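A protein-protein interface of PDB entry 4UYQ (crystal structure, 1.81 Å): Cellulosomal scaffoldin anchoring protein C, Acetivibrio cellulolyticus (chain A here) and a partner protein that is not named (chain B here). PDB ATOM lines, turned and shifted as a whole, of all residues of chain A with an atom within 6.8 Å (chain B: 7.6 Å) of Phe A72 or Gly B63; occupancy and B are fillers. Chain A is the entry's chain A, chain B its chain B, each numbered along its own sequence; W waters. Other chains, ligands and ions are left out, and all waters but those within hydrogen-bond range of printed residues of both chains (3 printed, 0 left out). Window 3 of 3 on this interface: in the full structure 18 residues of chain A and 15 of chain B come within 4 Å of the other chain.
Hydrophobic or aromatic side chains of chain A within 4 Å of the printed part of chain B: Tyr A65, Phe A72 and Tyr A118.
Hydrophobic or aromatic side chains of chain B within 4 Å of the printed part of chain A: Leu B62.
Among the printed residues, 11 pairs touch across the chains.
Among the printed residues, no Asp or Glu carboxylate lies within 4 Å of a Lys or Arg side-chain nitrogen of the other chain.
OD1 of Asn A115 sits at hydrogen-bond distance from N of Tyr A118 (3.4 Å).
The side-chain hydroxyl of Ser A74 is in hydrogen-bond range of the guanidinium group of Arg A37, 3.0 Å away.
O of Arg A37 lies within hydrogen-bond range of N of Asn A115, 2.9 Å away.
The backbone NH of Asn A67 sits at hydrogen-bond distance from the backbone carbonyl oxygen of Phe A72 (2.9 Å).
The backbone carbonyl oxygen (O) of Tyr A65 is in hydrogen-bond range of the backbone NH (N) of Ser A74 (2.6 Å).
NZ of Lys B64 lies within salt-bridge range of OD1 of Asp B59 (2.8 Å).
Water W1 lies within hydrogen-bond range of the backbone carbonyl oxygen of Tyr B60, the backbone carbonyl oxygen of Ile B65 and the side-chain hydroxyl of Tyr A118.
Water W2 lies within hydrogen-bond range of O of Gly B63, OH of Tyr A65 and ND2 of Asn A67.
Water W3 lies within hydrogen-bond range of the backbone carbonyl oxygen (O) of Val B61 (2.9 Å), the backbone carbonyl oxygen (O) of Tyr A118 (3.0 Å) and the side-chain hydroxyl (OG) of Ser A74 (3.5 Å).
Phe A72 touches just these residues of chain B: Leu B62 (3.4 Å) and Gly B63 (3.6 Å).
Gly B63 touches just these residues of chain A: Arg A37, Tyr A65 and Phe A72.
No residue of chain B comes within 4 Å of Gly A71.
Printed residues of chain A within 4 Å of Tyr B60: Tyr A118 (3.8 Å).
Of the printed residues of chain A, Lys B64 touches Tyr A65.
Of the printed residues of chain B, Arg A37 touches Val B61, Leu B62 and Gly B63.
Of the printed residues of chain A, Val B61 touches Arg A37 (3.0 Å) and Tyr A118 (3.5 Å).
Of the printed residues of chain B, Tyr A118 touches Tyr B60 and Val B61.
Asn A70 touches none of the printed residues of chain B.
The nearest residue of chain B that does not touch Phe A72 is Lys B64 (5.4 Å).
The nearest printed residue of chain A that does not touch Tyr B60 is Arg A37 (4.1 Å).
Arg A37 touches Leu B62.
Leu B62 touches Tyr A65 (O to CD2, 3.4 Å).
Tyr A65 touches Gly B63 (CE2 to O, 3.6 Å).
Lys B64 touches Tyr A65 (CG to CD1, 3.6 Å).
Phe A72 touches Leu B62 (CE1 to O, 3.4 Å).
Phe A72 touches Gly B63 (CZ to O, 3.6 Å).
Tyr A118 touches Tyr B60 (CE1 to O, 3.8 Å).
Tyr A118 touches Val B61 (CD1 to O, 3.5 Å).
NH2 of Arg A37 lies close to N of Gly B63 (3.3 Å).
O of Leu B62 lies within hydrogen-bond range of OG of Ser A74, 2.8 Å away.
NH2 of Arg A37 lies within hydrogen-bond range of O of Val B61 (3.0 Å).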
ATOM      1  N   ARG A  37       3.861 -16.866  22.429  1.00  0.00           N
ATOM      2  CA  ARG A  37       2.810 -16.093  21.829  1.00  0.00           C
ATOM      3  C   ARG A  37       3.210 -15.684  20.408  1.00  0.00           C
ATOM      4  O   ARG A  37       4.398 -15.251  20.216  1.00  0.00           O
ATOM      5  CB  ARG A  37       2.589 -14.852  22.610  1.00  0.00           C
ATOM      6  CG  ARG A  37       1.491 -14.031  21.961  1.00  0.00           C
ATOM      7  CD  ARG A  37       0.921 -12.890  22.690  1.00  0.00           C
ATOM      8  NE  ARG A  37       0.415 -13.175  24.020  1.00  0.00           N
ATOM      9  CZ  ARG A  37      -0.162 -12.227  24.728  1.00  0.00           C
ATOM     10  NH1 ARG A  37      -0.371 -11.073  24.147  1.00  0.00           N
ATOM     11  NH2 ARG A  37      -0.547 -12.436  25.988  1.00  0.00           N
ATOM     12  N   THR A  38       2.310 -15.888  19.464  1.00  0.00           N
ATOM     13  CA  THR A  38       2.534 -15.494  18.084  1.00  0.00           C
ATOM     14  C   THR A  38       1.616 -14.365  17.749  1.00  0.00           C
ATOM     15  O   THR A  38       0.421 -14.449  18.055  1.00  0.00           O
ATOM     16  CB  THR A  38       2.215 -16.646  17.066  1.00  0.00           C
ATOM     17  OG1 THR A  38       0.851 -17.048  17.149  1.00  0.00           O
ATOM     18  CG2 THR A  38       2.945 -17.798  17.364  1.00  0.00           C
ATOM     19  N   ASN A  39       2.114 -13.372  17.050  1.00  0.00           N
ATOM     20  CA  ASN A  39       1.308 -12.284  16.497  1.00  0.00           C
ATOM     21  C   ASN A  39       1.081 -12.471  15.011  1.00  0.00           C
ATOM     22  O   ASN A  39       1.880 -13.036  14.328  1.00  0.00           O
ATOM     23  CB  ASN A  39       2.025 -10.967  16.695  1.00  0.00           C
ATOM     24  CG  ASN A  39       2.016 -10.568  18.151  1.00  0.00           C
ATOM     25  OD1 ASN A  39       3.024 -10.508  18.758  1.00  0.00           O
ATOM     26  ND2 ASN A  39       0.871 -10.340  18.694  1.00  0.00           N
ATOM     27  N   PHE A  40      -0.054 -11.997  14.544  1.00  0.00           N
ATOM     28  CA  PHE A  40      -0.453 -12.041  13.181  1.00  0.00           C
ATOM     29  C   PHE A  40      -1.374 -10.883  12.851  1.00  0.00           C
ATOM     30  O   PHE A  40      -1.920 -10.228  13.774  1.00  0.00           O
ATOM     31  CB  PHE A  40      -1.150 -13.358  12.832  1.00  0.00           C
ATOM     32  CG  PHE A  40      -2.347 -13.686  13.671  1.00  0.00           C
ATOM     33  CD1 PHE A  40      -2.194 -14.417  14.842  1.00  0.00           C
ATOM     34  CD2 PHE A  40      -3.593 -13.327  13.289  1.00  0.00           C
ATOM     35  CE1 PHE A  40      -3.269 -14.714  15.634  1.00  0.00           C
ATOM     36  CE2 PHE A  40      -4.709 -13.650  14.055  1.00  0.00           C
ATOM     37  CZ  PHE A  40      -4.563 -14.331  15.243  1.00  0.00           C
ATOM     38  N   PRO A  42      -4.820  -9.833  11.793  1.00  0.00           N
ATOM     39  CA  PRO A  42      -6.124 -10.466  11.678  1.00  0.00           C
ATOM     40  C   PRO A  42      -6.966 -10.094  10.447  1.00  0.00           C
ATOM     41  O   PRO A  42      -7.956 -10.786  10.179  1.00  0.00           O
ATOM     42  CB  PRO A  42      -6.812 -10.097  12.979  1.00  0.00           C
ATOM     43  CG  PRO A  42      -6.096  -8.925  13.466  1.00  0.00           C
ATOM     44  CD  PRO A  42      -4.775  -8.811  12.852  1.00  0.00           C
ATOM     45  N   VAL A  47      -7.024 -17.313  13.795  1.00  0.00           N
ATOM     46  CA  VAL A  47      -6.927 -18.626  14.379  1.00  0.00           C
ATOM     47  C   VAL A  47      -8.256 -19.396  14.375  1.00  0.00           C
ATOM     48  O   VAL A  47      -9.259 -18.891  14.886  1.00  0.00           O
ATOM     49  CB  VAL A  47      -6.415 -18.508  15.814  1.00  0.00           C
ATOM     50  CG1 VAL A  47      -6.206 -19.862  16.401  1.00  0.00           C
ATOM     51  CG2 VAL A  47      -5.038 -17.851  15.776  1.00  0.00           C
ATOM     52  N   ILE A  50      -6.139 -24.375  18.086  1.00  0.00           N
ATOM     53  CA  ILE A  50      -4.775 -24.745  18.421  1.00  0.00           C
ATOM     54  C   ILE A  50      -4.853 -26.161  18.982  1.00  0.00           C
ATOM     55  O   ILE A  50      -5.641 -26.420  19.929  1.00  0.00           O
ATOM     56  CB  ILE A  50      -4.132 -23.766  19.462  1.00  0.00           C
ATOM     57  CG1 ILE A  50      -4.144 -22.338  18.943  1.00  0.00           C
ATOM     58  CG2 ILE A  50      -2.769 -24.191  19.902  1.00  0.00           C
ATOM     59  CD1 ILE A  50      -3.936 -21.231  19.981  1.00  0.00           C
ATOM     60  N   TYR A  65      -4.957 -20.045  24.133  1.00  0.00           N
ATOM     61  CA  TYR A  65      -5.913 -18.979  23.966  1.00  0.00           C
ATOM     62  C   TYR A  65      -5.528 -18.263  22.703  1.00  0.00           C
ATOM     63  O   TYR A  65      -4.351 -18.266  22.329  1.00  0.00           O
ATOM     64  CB  TYR A  65      -5.810 -18.016  25.154  1.00  0.00           C
ATOM     65  CG  TYR A  65      -6.770 -16.883  25.101  1.00  0.00           C
ATOM     66  CD1 TYR A  65      -8.164 -17.106  25.220  1.00  0.00           C
ATOM     67  CD2 TYR A  65      -6.326 -15.575  24.945  1.00  0.00           C
ATOM     68  CE1 TYR A  65      -9.070 -16.050  25.191  1.00  0.00           C
ATOM     69  CE2 TYR A  65      -7.199 -14.517  24.875  1.00  0.00           C
ATOM     70  CZ  TYR A  65      -8.575 -14.749  25.044  1.00  0.00           C
ATOM     71  OH  TYR A  65      -9.493 -13.753  25.034  1.00  0.00           O
ATOM     72  N   TYR A  66      -6.500 -17.643  22.047  1.00  0.00           N
ATOM     73  CA  TYR A  66      -6.234 -16.775  20.936  1.00  0.00           C
ATOM     74  C   TYR A  66      -7.239 -15.649  20.938  1.00  0.00           C
ATOM     75  O   TYR A  66      -8.377 -15.759  21.499  1.00  0.00           O
ATOM     76  CB  TYR A  66      -6.340 -17.503  19.612  1.00  0.00           C
ATOM     77  CG  TYR A  66      -7.616 -18.268  19.364  1.00  0.00           C
ATOM     78  CD1 TYR A  66      -8.706 -17.649  18.763  1.00  0.00           C
ATOM     79  CD2 TYR A  66      -7.731 -19.621  19.693  1.00  0.00           C
ATOM     80  CE1 TYR A  66      -9.907 -18.352  18.507  1.00  0.00           C
ATOM     81  CE2 TYR A  66      -8.933 -20.323  19.472  1.00  0.00           C
ATOM     82  CZ  TYR A  66     -10.011 -19.659  18.874  1.00  0.00           C
ATOM     83  OH  TYR A  66     -11.222 -20.274  18.558  1.00  0.00           O
ATOM     84  N   ASN A  67      -6.819 -14.587  20.299  1.00  0.00           N
ATOM     85  CA  ASN A  67      -7.627 -13.345  20.160  1.00  0.00           C
ATOM     86  C   ASN A  67      -7.555 -12.883  18.689  1.00  0.00           C
ATOM     87  O   ASN A  67      -6.503 -12.383  18.246  1.00  0.00           O
ATOM     88  CB  ASN A  67      -7.061 -12.292  21.141  1.00  0.00           C
ATOM     89  CG  ASN A  67      -7.838 -10.975  21.100  1.00  0.00           C
ATOM     90  OD1 ASN A  67      -8.414 -10.614  20.073  1.00  0.00           O
ATOM     91  ND2 ASN A  67      -7.816 -10.251  22.209  1.00  0.00           N
ATOM     92  N   ASN A  68      -8.653 -13.068  17.948  1.00  0.00           N
ATOM     93  CA  ASN A  68      -8.739 -12.719  16.551  1.00  0.00           C
ATOM     94  C   ASN A  68      -9.098 -11.319  16.259  1.00  0.00           C
ATOM     95  O   ASN A  68      -9.083 -10.905  15.123  1.00  0.00           O
ATOM     96  CB  ASN A  68      -9.703 -13.661  15.804  1.00  0.00           C
ATOM     97  CG  ASN A  68      -9.101 -15.002  15.586  1.00  0.00           C
ATOM     98  OD1 ASN A  68      -7.874 -15.134  15.466  1.00  0.00           O
ATOM     99  ND2 ASN A  68      -9.928 -16.010  15.609  1.00  0.00           N
ATOM    100  N   GLU A  69      -9.319 -10.538  17.308  1.00  0.00           N
ATOM    101  CA  GLU A  69      -9.458  -9.096  17.241  1.00  0.00           C
ATOM    102  C   GLU A  69      -8.126  -8.368  17.247  1.00  0.00           C
ATOM    103  O   GLU A  69      -7.848  -7.544  16.403  1.00  0.00           O
ATOM    104  CB  GLU A  69     -10.319  -8.616  18.425  1.00  0.00           C
ATOM    105  CG  GLU A  69     -10.449  -7.109  18.519  1.00  0.00           C
ATOM    106  CD  GLU A  69     -11.314  -6.478  17.416  1.00  0.00           C
ATOM    107  OE1 GLU A  69     -12.088  -7.190  16.732  1.00  0.00           O
ATOM    108  OE2 GLU A  69     -11.204  -5.238  17.229  1.00  0.00           O
ATOM    109  N   ASN A  70      -7.309  -8.582  18.259  1.00  0.00           N
ATOM    110  CA  ASN A  70      -5.999  -8.002  18.300  1.00  0.00           C
ATOM    111  C   ASN A  70      -4.879  -8.827  17.643  1.00  0.00           C
ATOM    112  O   ASN A  70      -3.793  -8.326  17.539  1.00  0.00           O
ATOM    113  CB  ASN A  70      -5.648  -7.791  19.763  1.00  0.00           C
ATOM    114  CG  ASN A  70      -6.596  -6.815  20.436  1.00  0.00           C
ATOM    115  OD1 ASN A  70      -7.524  -7.185  21.178  1.00  0.00           O
ATOM    116  ND2 ASN A  70      -6.389  -5.568  20.124  1.00  0.00           N
ATOM    117  N   GLY A  71      -5.121 -10.074  17.274  1.00  0.00           N
ATOM    118  CA  GLY A  71      -4.144 -10.844  16.468  1.00  0.00           C
ATOM    119  C   GLY A  71      -3.028 -11.532  17.211  1.00  0.00           C
ATOM    120  O   GLY A  71      -1.818 -11.309  16.952  1.00  0.00           O
ATOM    121  N   PHE A  72      -3.384 -12.390  18.158  1.00  0.00           N
ATOM    122  CA  PHE A  72      -2.367 -13.271  18.784  1.00  0.00           C
ATOM    123  C   PHE A  72      -2.924 -14.584  19.183  1.00  0.00           C
ATOM    124  O   PHE A  72      -4.149 -14.759  19.309  1.00  0.00           O
ATOM    125  CB  PHE A  72      -1.672 -12.525  19.980  1.00  0.00           C
ATOM    126  CG  PHE A  72      -2.564 -12.239  21.141  1.00  0.00           C
ATOM    127  CD1 PHE A  72      -2.774 -13.222  22.079  1.00  0.00           C
ATOM    128  CD2 PHE A  72      -3.183 -10.960  21.336  1.00  0.00           C
ATOM    129  CE1 PHE A  72      -3.605 -12.980  23.191  1.00  0.00           C
ATOM    130  CE2 PHE A  72      -4.041 -10.744  22.430  1.00  0.00           C
ATOM    131  CZ  PHE A  72      -4.235 -11.762  23.347  1.00  0.00           C
ATOM    132  N   ALA A  73      -2.012 -15.562  19.265  1.00  0.00           N
ATOM    133  CA  ALA A  73      -2.323 -16.882  19.647  1.00  0.00           C
ATOM    134  C   ALA A  73      -1.222 -17.091  20.574  1.00  0.00           C
ATOM    135  O   ALA A  73      -0.046 -16.833  20.586  1.00  0.00           O
ATOM    136  CB  ALA A  73      -2.229 -17.908  18.568  1.00  0.00           C
ATOM    137  N   SER A  74      -1.798 -17.823  22.143  1.00  0.00           N
ATOM    138  CA  SER A  74      -0.848 -18.046  23.191  1.00  0.00           C
ATOM    139  C   SER A  74      -0.976 -19.469  23.601  1.00  0.00           C
ATOM    140  O   SER A  74      -2.074 -20.063  23.523  1.00  0.00           O
ATOM    141  CB  SER A  74      -1.221 -17.124  24.358  1.00  0.00           C
ATOM    142  OG  SER A  74      -1.132 -15.759  24.003  1.00  0.00           O
ATOM    143  N   ASN A 115       6.165 -13.065  19.714  1.00  0.00           N
ATOM    144  CA  ASN A 115       6.028 -11.899  20.577  1.00  0.00           C
ATOM    145  C   ASN A 115       6.971 -12.022  21.746  1.00  0.00           C
ATOM    146  O   ASN A 115       6.740 -12.855  22.601  1.00  0.00           O
ATOM    147  CB  ASN A 115       4.594 -11.823  21.072  1.00  0.00           C
ATOM    148  CG  ASN A 115       4.343 -10.523  21.835  1.00  0.00           C
ATOM    149  OD1 ASN A 115       5.057 -10.228  22.806  1.00  0.00           O
ATOM    150  ND2 ASN A 115       3.367  -9.761  21.425  1.00  0.00           N
ATOM    151  N   TYR A 118       5.706 -11.886  25.742  1.00  0.00           N
ATOM    152  CA  TYR A 118       4.864 -12.913  26.255  1.00  0.00           C
ATOM    153  C   TYR A 118       5.369 -14.339  25.996  1.00  0.00           C
ATOM    154  O   TYR A 118       4.599 -15.321  26.046  1.00  0.00           O
ATOM    155  CB  TYR A 118       3.501 -12.695  25.697  1.00  0.00           C
ATOM    156  CG  TYR A 118       2.799 -11.519  26.320  1.00  0.00           C
ATOM    157  CD1 TYR A 118       2.145 -11.691  27.523  1.00  0.00           C
ATOM    158  CD2 TYR A 118       2.661 -10.287  25.659  1.00  0.00           C
ATOM    159  CE1 TYR A 118       1.411 -10.660  28.116  1.00  0.00           C
ATOM    160  CE2 TYR A 118       1.950  -9.214  26.257  1.00  0.00           C
ATOM    161  CZ  TYR A 118       1.305  -9.418  27.478  1.00  0.00           C
ATOM    162  OH  TYR A 118       0.551  -8.417  28.128  1.00  0.00           O
ATOM    163  N   VAL B  57      -2.577 -15.506  37.100  1.00  0.00           N
ATOM    164  CA  VAL B  57      -1.266 -15.120  36.487  1.00  0.00           C
ATOM    165  C   VAL B  57      -1.060 -15.839  35.110  1.00  0.00           C
ATOM    166  O   VAL B  57      -0.695 -15.177  34.098  1.00  0.00           O
ATOM    167  CB  VAL B  57      -0.065 -15.293  37.421  1.00  0.00           C
ATOM    168  CG1 VAL B  57       1.252 -14.960  36.673  1.00  0.00           C
ATOM    169  CG2 VAL B  57      -0.222 -14.451  38.657  1.00  0.00           C
ATOM    170  N   ARG B  58      -1.331 -17.147  35.035  1.00  0.00           N
ATOM    171  CA  ARG B  58      -1.359 -17.805  33.717  1.00  0.00           C
ATOM    172  C   ARG B  58      -2.287 -17.106  32.717  1.00  0.00           C
ATOM    173  O   ARG B  58      -1.911 -16.873  31.553  1.00  0.00           O
ATOM    174  CB  ARG B  58      -1.623 -19.290  33.806  1.00  0.00           C
ATOM    175  CG  ARG B  58      -1.534 -19.989  32.441  1.00  0.00           C
ATOM    176  CD  ARG B  58      -1.848 -21.453  32.712  1.00  0.00           C
ATOM    177  NE  ARG B  58      -3.221 -21.635  32.996  1.00  0.00           N
ATOM    178  CZ  ARG B  58      -3.745 -22.650  33.708  1.00  0.00           C
ATOM    179  NH1 ARG B  58      -3.048 -23.653  34.202  1.00  0.00           N
ATOM    180  NH2 ARG B  58      -5.032 -22.668  33.886  1.00  0.00           N
ATOM    181  N   ASP B  59      -3.513 -16.754  33.134  1.00  0.00           N
ATOM    182  CA  ASP B  59      -4.439 -16.018  32.252  1.00  0.00           C
ATOM    183  C   ASP B  59      -3.881 -14.670  31.732  1.00  0.00           C
ATOM    184  O   ASP B  59      -4.150 -14.305  30.607  1.00  0.00           O
ATOM    185  CB  ASP B  59      -5.775 -15.729  32.959  1.00  0.00           C
ATOM    186  CG  ASP B  59      -6.659 -17.005  33.133  1.00  0.00           C
ATOM    187  OD1 ASP B  59      -6.378 -18.038  32.512  1.00  0.00           O
ATOM    188  OD2 ASP B  59      -7.647 -16.950  33.938  1.00  0.00           O
ATOM    189  N   TYR B  60      -3.153 -13.950  32.605  1.00  0.00           N
ATOM    190  CA  TYR B  60      -2.417 -12.763  32.164  1.00  0.00           C
ATOM    191  C   TYR B  60      -1.432 -13.058  31.055  1.00  0.00           C
ATOM    192  O   TYR B  60      -1.422 -12.421  29.993  1.00  0.00           O
ATOM    193  CB  TYR B  60      -1.783 -12.074  33.343  1.00  0.00           C
ATOM    194  CG  TYR B  60      -1.127 -10.788  33.005  1.00  0.00           C
ATOM    195  CD1 TYR B  60       0.168 -10.769  32.514  1.00  0.00           C
ATOM    196  CD2 TYR B  60      -1.833  -9.567  33.180  1.00  0.00           C
ATOM    197  CE1 TYR B  60       0.753  -9.554  32.126  1.00  0.00           C
ATOM    198  CE2 TYR B  60      -1.246  -8.363  32.852  1.00  0.00           C
ATOM    199  CZ  TYR B  60       0.049  -8.381  32.312  1.00  0.00           C
ATOM    200  OH  TYR B  60       0.600  -7.173  31.999  1.00  0.00           O
ATOM    201  N   VAL B  61      -0.624 -14.059  31.274  1.00  0.00           N
ATOM    202  CA  VAL B  61       0.354 -14.479  30.282  1.00  0.00           C
ATOM    203  C   VAL B  61      -0.283 -14.927  28.953  1.00  0.00           C
ATOM    204  O   VAL B  61       0.272 -14.566  27.929  1.00  0.00           O
ATOM    205  CB  VAL B  61       1.291 -15.526  30.900  1.00  0.00           C
ATOM    206  CG1 VAL B  61       2.278 -16.014  29.824  1.00  0.00           C
ATOM    207  CG2 VAL B  61       2.029 -14.956  32.101  1.00  0.00           C
ATOM    208  N   LEU B  62      -1.415 -15.640  28.980  1.00  0.00           N
ATOM    209  CA  LEU B  62      -2.164 -16.064  27.838  1.00  0.00           C
ATOM    210  C   LEU B  62      -2.785 -14.903  27.106  1.00  0.00           C
ATOM    211  O   LEU B  62      -3.114 -15.012  25.907  1.00  0.00           O
ATOM    212  CB  LEU B  62      -3.219 -17.074  28.191  1.00  0.00           C
ATOM    213  CG  LEU B  62      -2.735 -18.465  28.649  1.00  0.00           C
ATOM    214  CD1 LEU B  62      -3.812 -19.256  29.339  1.00  0.00           C
ATOM    215  CD2 LEU B  62      -2.322 -19.208  27.401  1.00  0.00           C
ATOM    216  N   GLY B  63      -2.955 -13.783  27.837  1.00  0.00           N
ATOM    217  CA  GLY B  63      -3.547 -12.625  27.217  1.00  0.00           C
ATOM    218  C   GLY B  63      -5.046 -12.592  27.343  1.00  0.00           C
ATOM    219  O   GLY B  63      -5.744 -11.774  26.652  1.00  0.00           O
ATOM    220  N   LYS B  64      -5.593 -13.386  28.275  1.00  0.00           N
ATOM    221  CA  LYS B  64      -7.066 -13.368  28.556  1.00  0.00           C
ATOM    222  C   LYS B  64      -7.510 -12.124  29.318  1.00  0.00           C
ATOM    223  O   LYS B  64      -8.639 -11.618  29.137  1.00  0.00           O
ATOM    224  CB  LYS B  64      -7.502 -14.576  29.351  1.00  0.00           C
ATOM    225  CG  LYS B  64      -7.461 -15.886  28.582  1.00  0.00           C
ATOM    226  CD  LYS B  64      -8.398 -16.839  29.214  1.00  0.00           C
ATOM    227  CE  LYS B  64      -7.693 -17.862  29.970  1.00  0.00           C
ATOM    228  NZ  LYS B  64      -8.670 -18.372  31.023  1.00  0.00           N
ATOM    229  N   ILE B  65      -6.620 -11.593  30.111  1.00  0.00           N
ATOM    230  CA  ILE B  65      -6.873 -10.459  30.915  1.00  0.00           C
ATOM    231  C   ILE B  65      -5.670  -9.531  30.987  1.00  0.00           C
ATOM    232  O   ILE B  65      -4.500  -9.965  30.823  1.00  0.00           O
ATOM    233  CB  ILE B  65      -7.200 -10.836  32.401  1.00  0.00           C
ATOM    234  CG1 ILE B  65      -6.014 -11.520  33.132  1.00  0.00           C
ATOM    235  CG2 ILE B  65      -8.459 -11.681  32.495  1.00  0.00           C
ATOM    236  CD1 ILE B  65      -6.219 -11.819  34.624  1.00  0.00           C
ATOM    237  N   PHE B  66      -5.977  -8.232  31.225  1.00  0.00           N
ATOM    238  CA  PHE B  66      -4.968  -7.237  31.547  1.00  0.00           C
ATOM    239  C   PHE B  66      -5.002  -6.776  32.992  1.00  0.00           C
ATOM    240  O   PHE B  66      -3.985  -6.383  33.521  1.00  0.00           O
ATOM    241  CB  PHE B  66      -5.133  -6.003  30.704  1.00  0.00           C
ATOM    242  CG  PHE B  66      -4.733  -6.168  29.269  1.00  0.00           C
ATOM    243  CD1 PHE B  66      -3.412  -6.365  28.923  1.00  0.00           C
ATOM    244  CD2 PHE B  66      -5.677  -5.942  28.272  1.00  0.00           C
ATOM    245  CE1 PHE B  66      -3.040  -6.437  27.588  1.00  0.00           C
ATOM    246  CE2 PHE B  66      -5.309  -6.023  26.941  1.00  0.00           C
ATOM    247  CZ  PHE B  66      -3.986  -6.257  26.618  1.00  0.00           C
HETATM  248  O   HOH W   1      -2.095  -9.788  29.347  1.00  0.00           O
HETATM  249  O   HOH W   2      -7.993 -11.165  25.108  1.00  0.00           O
HETATM  250  O   HOH W   3       1.758 -16.137  25.940  1.00  0.00           O
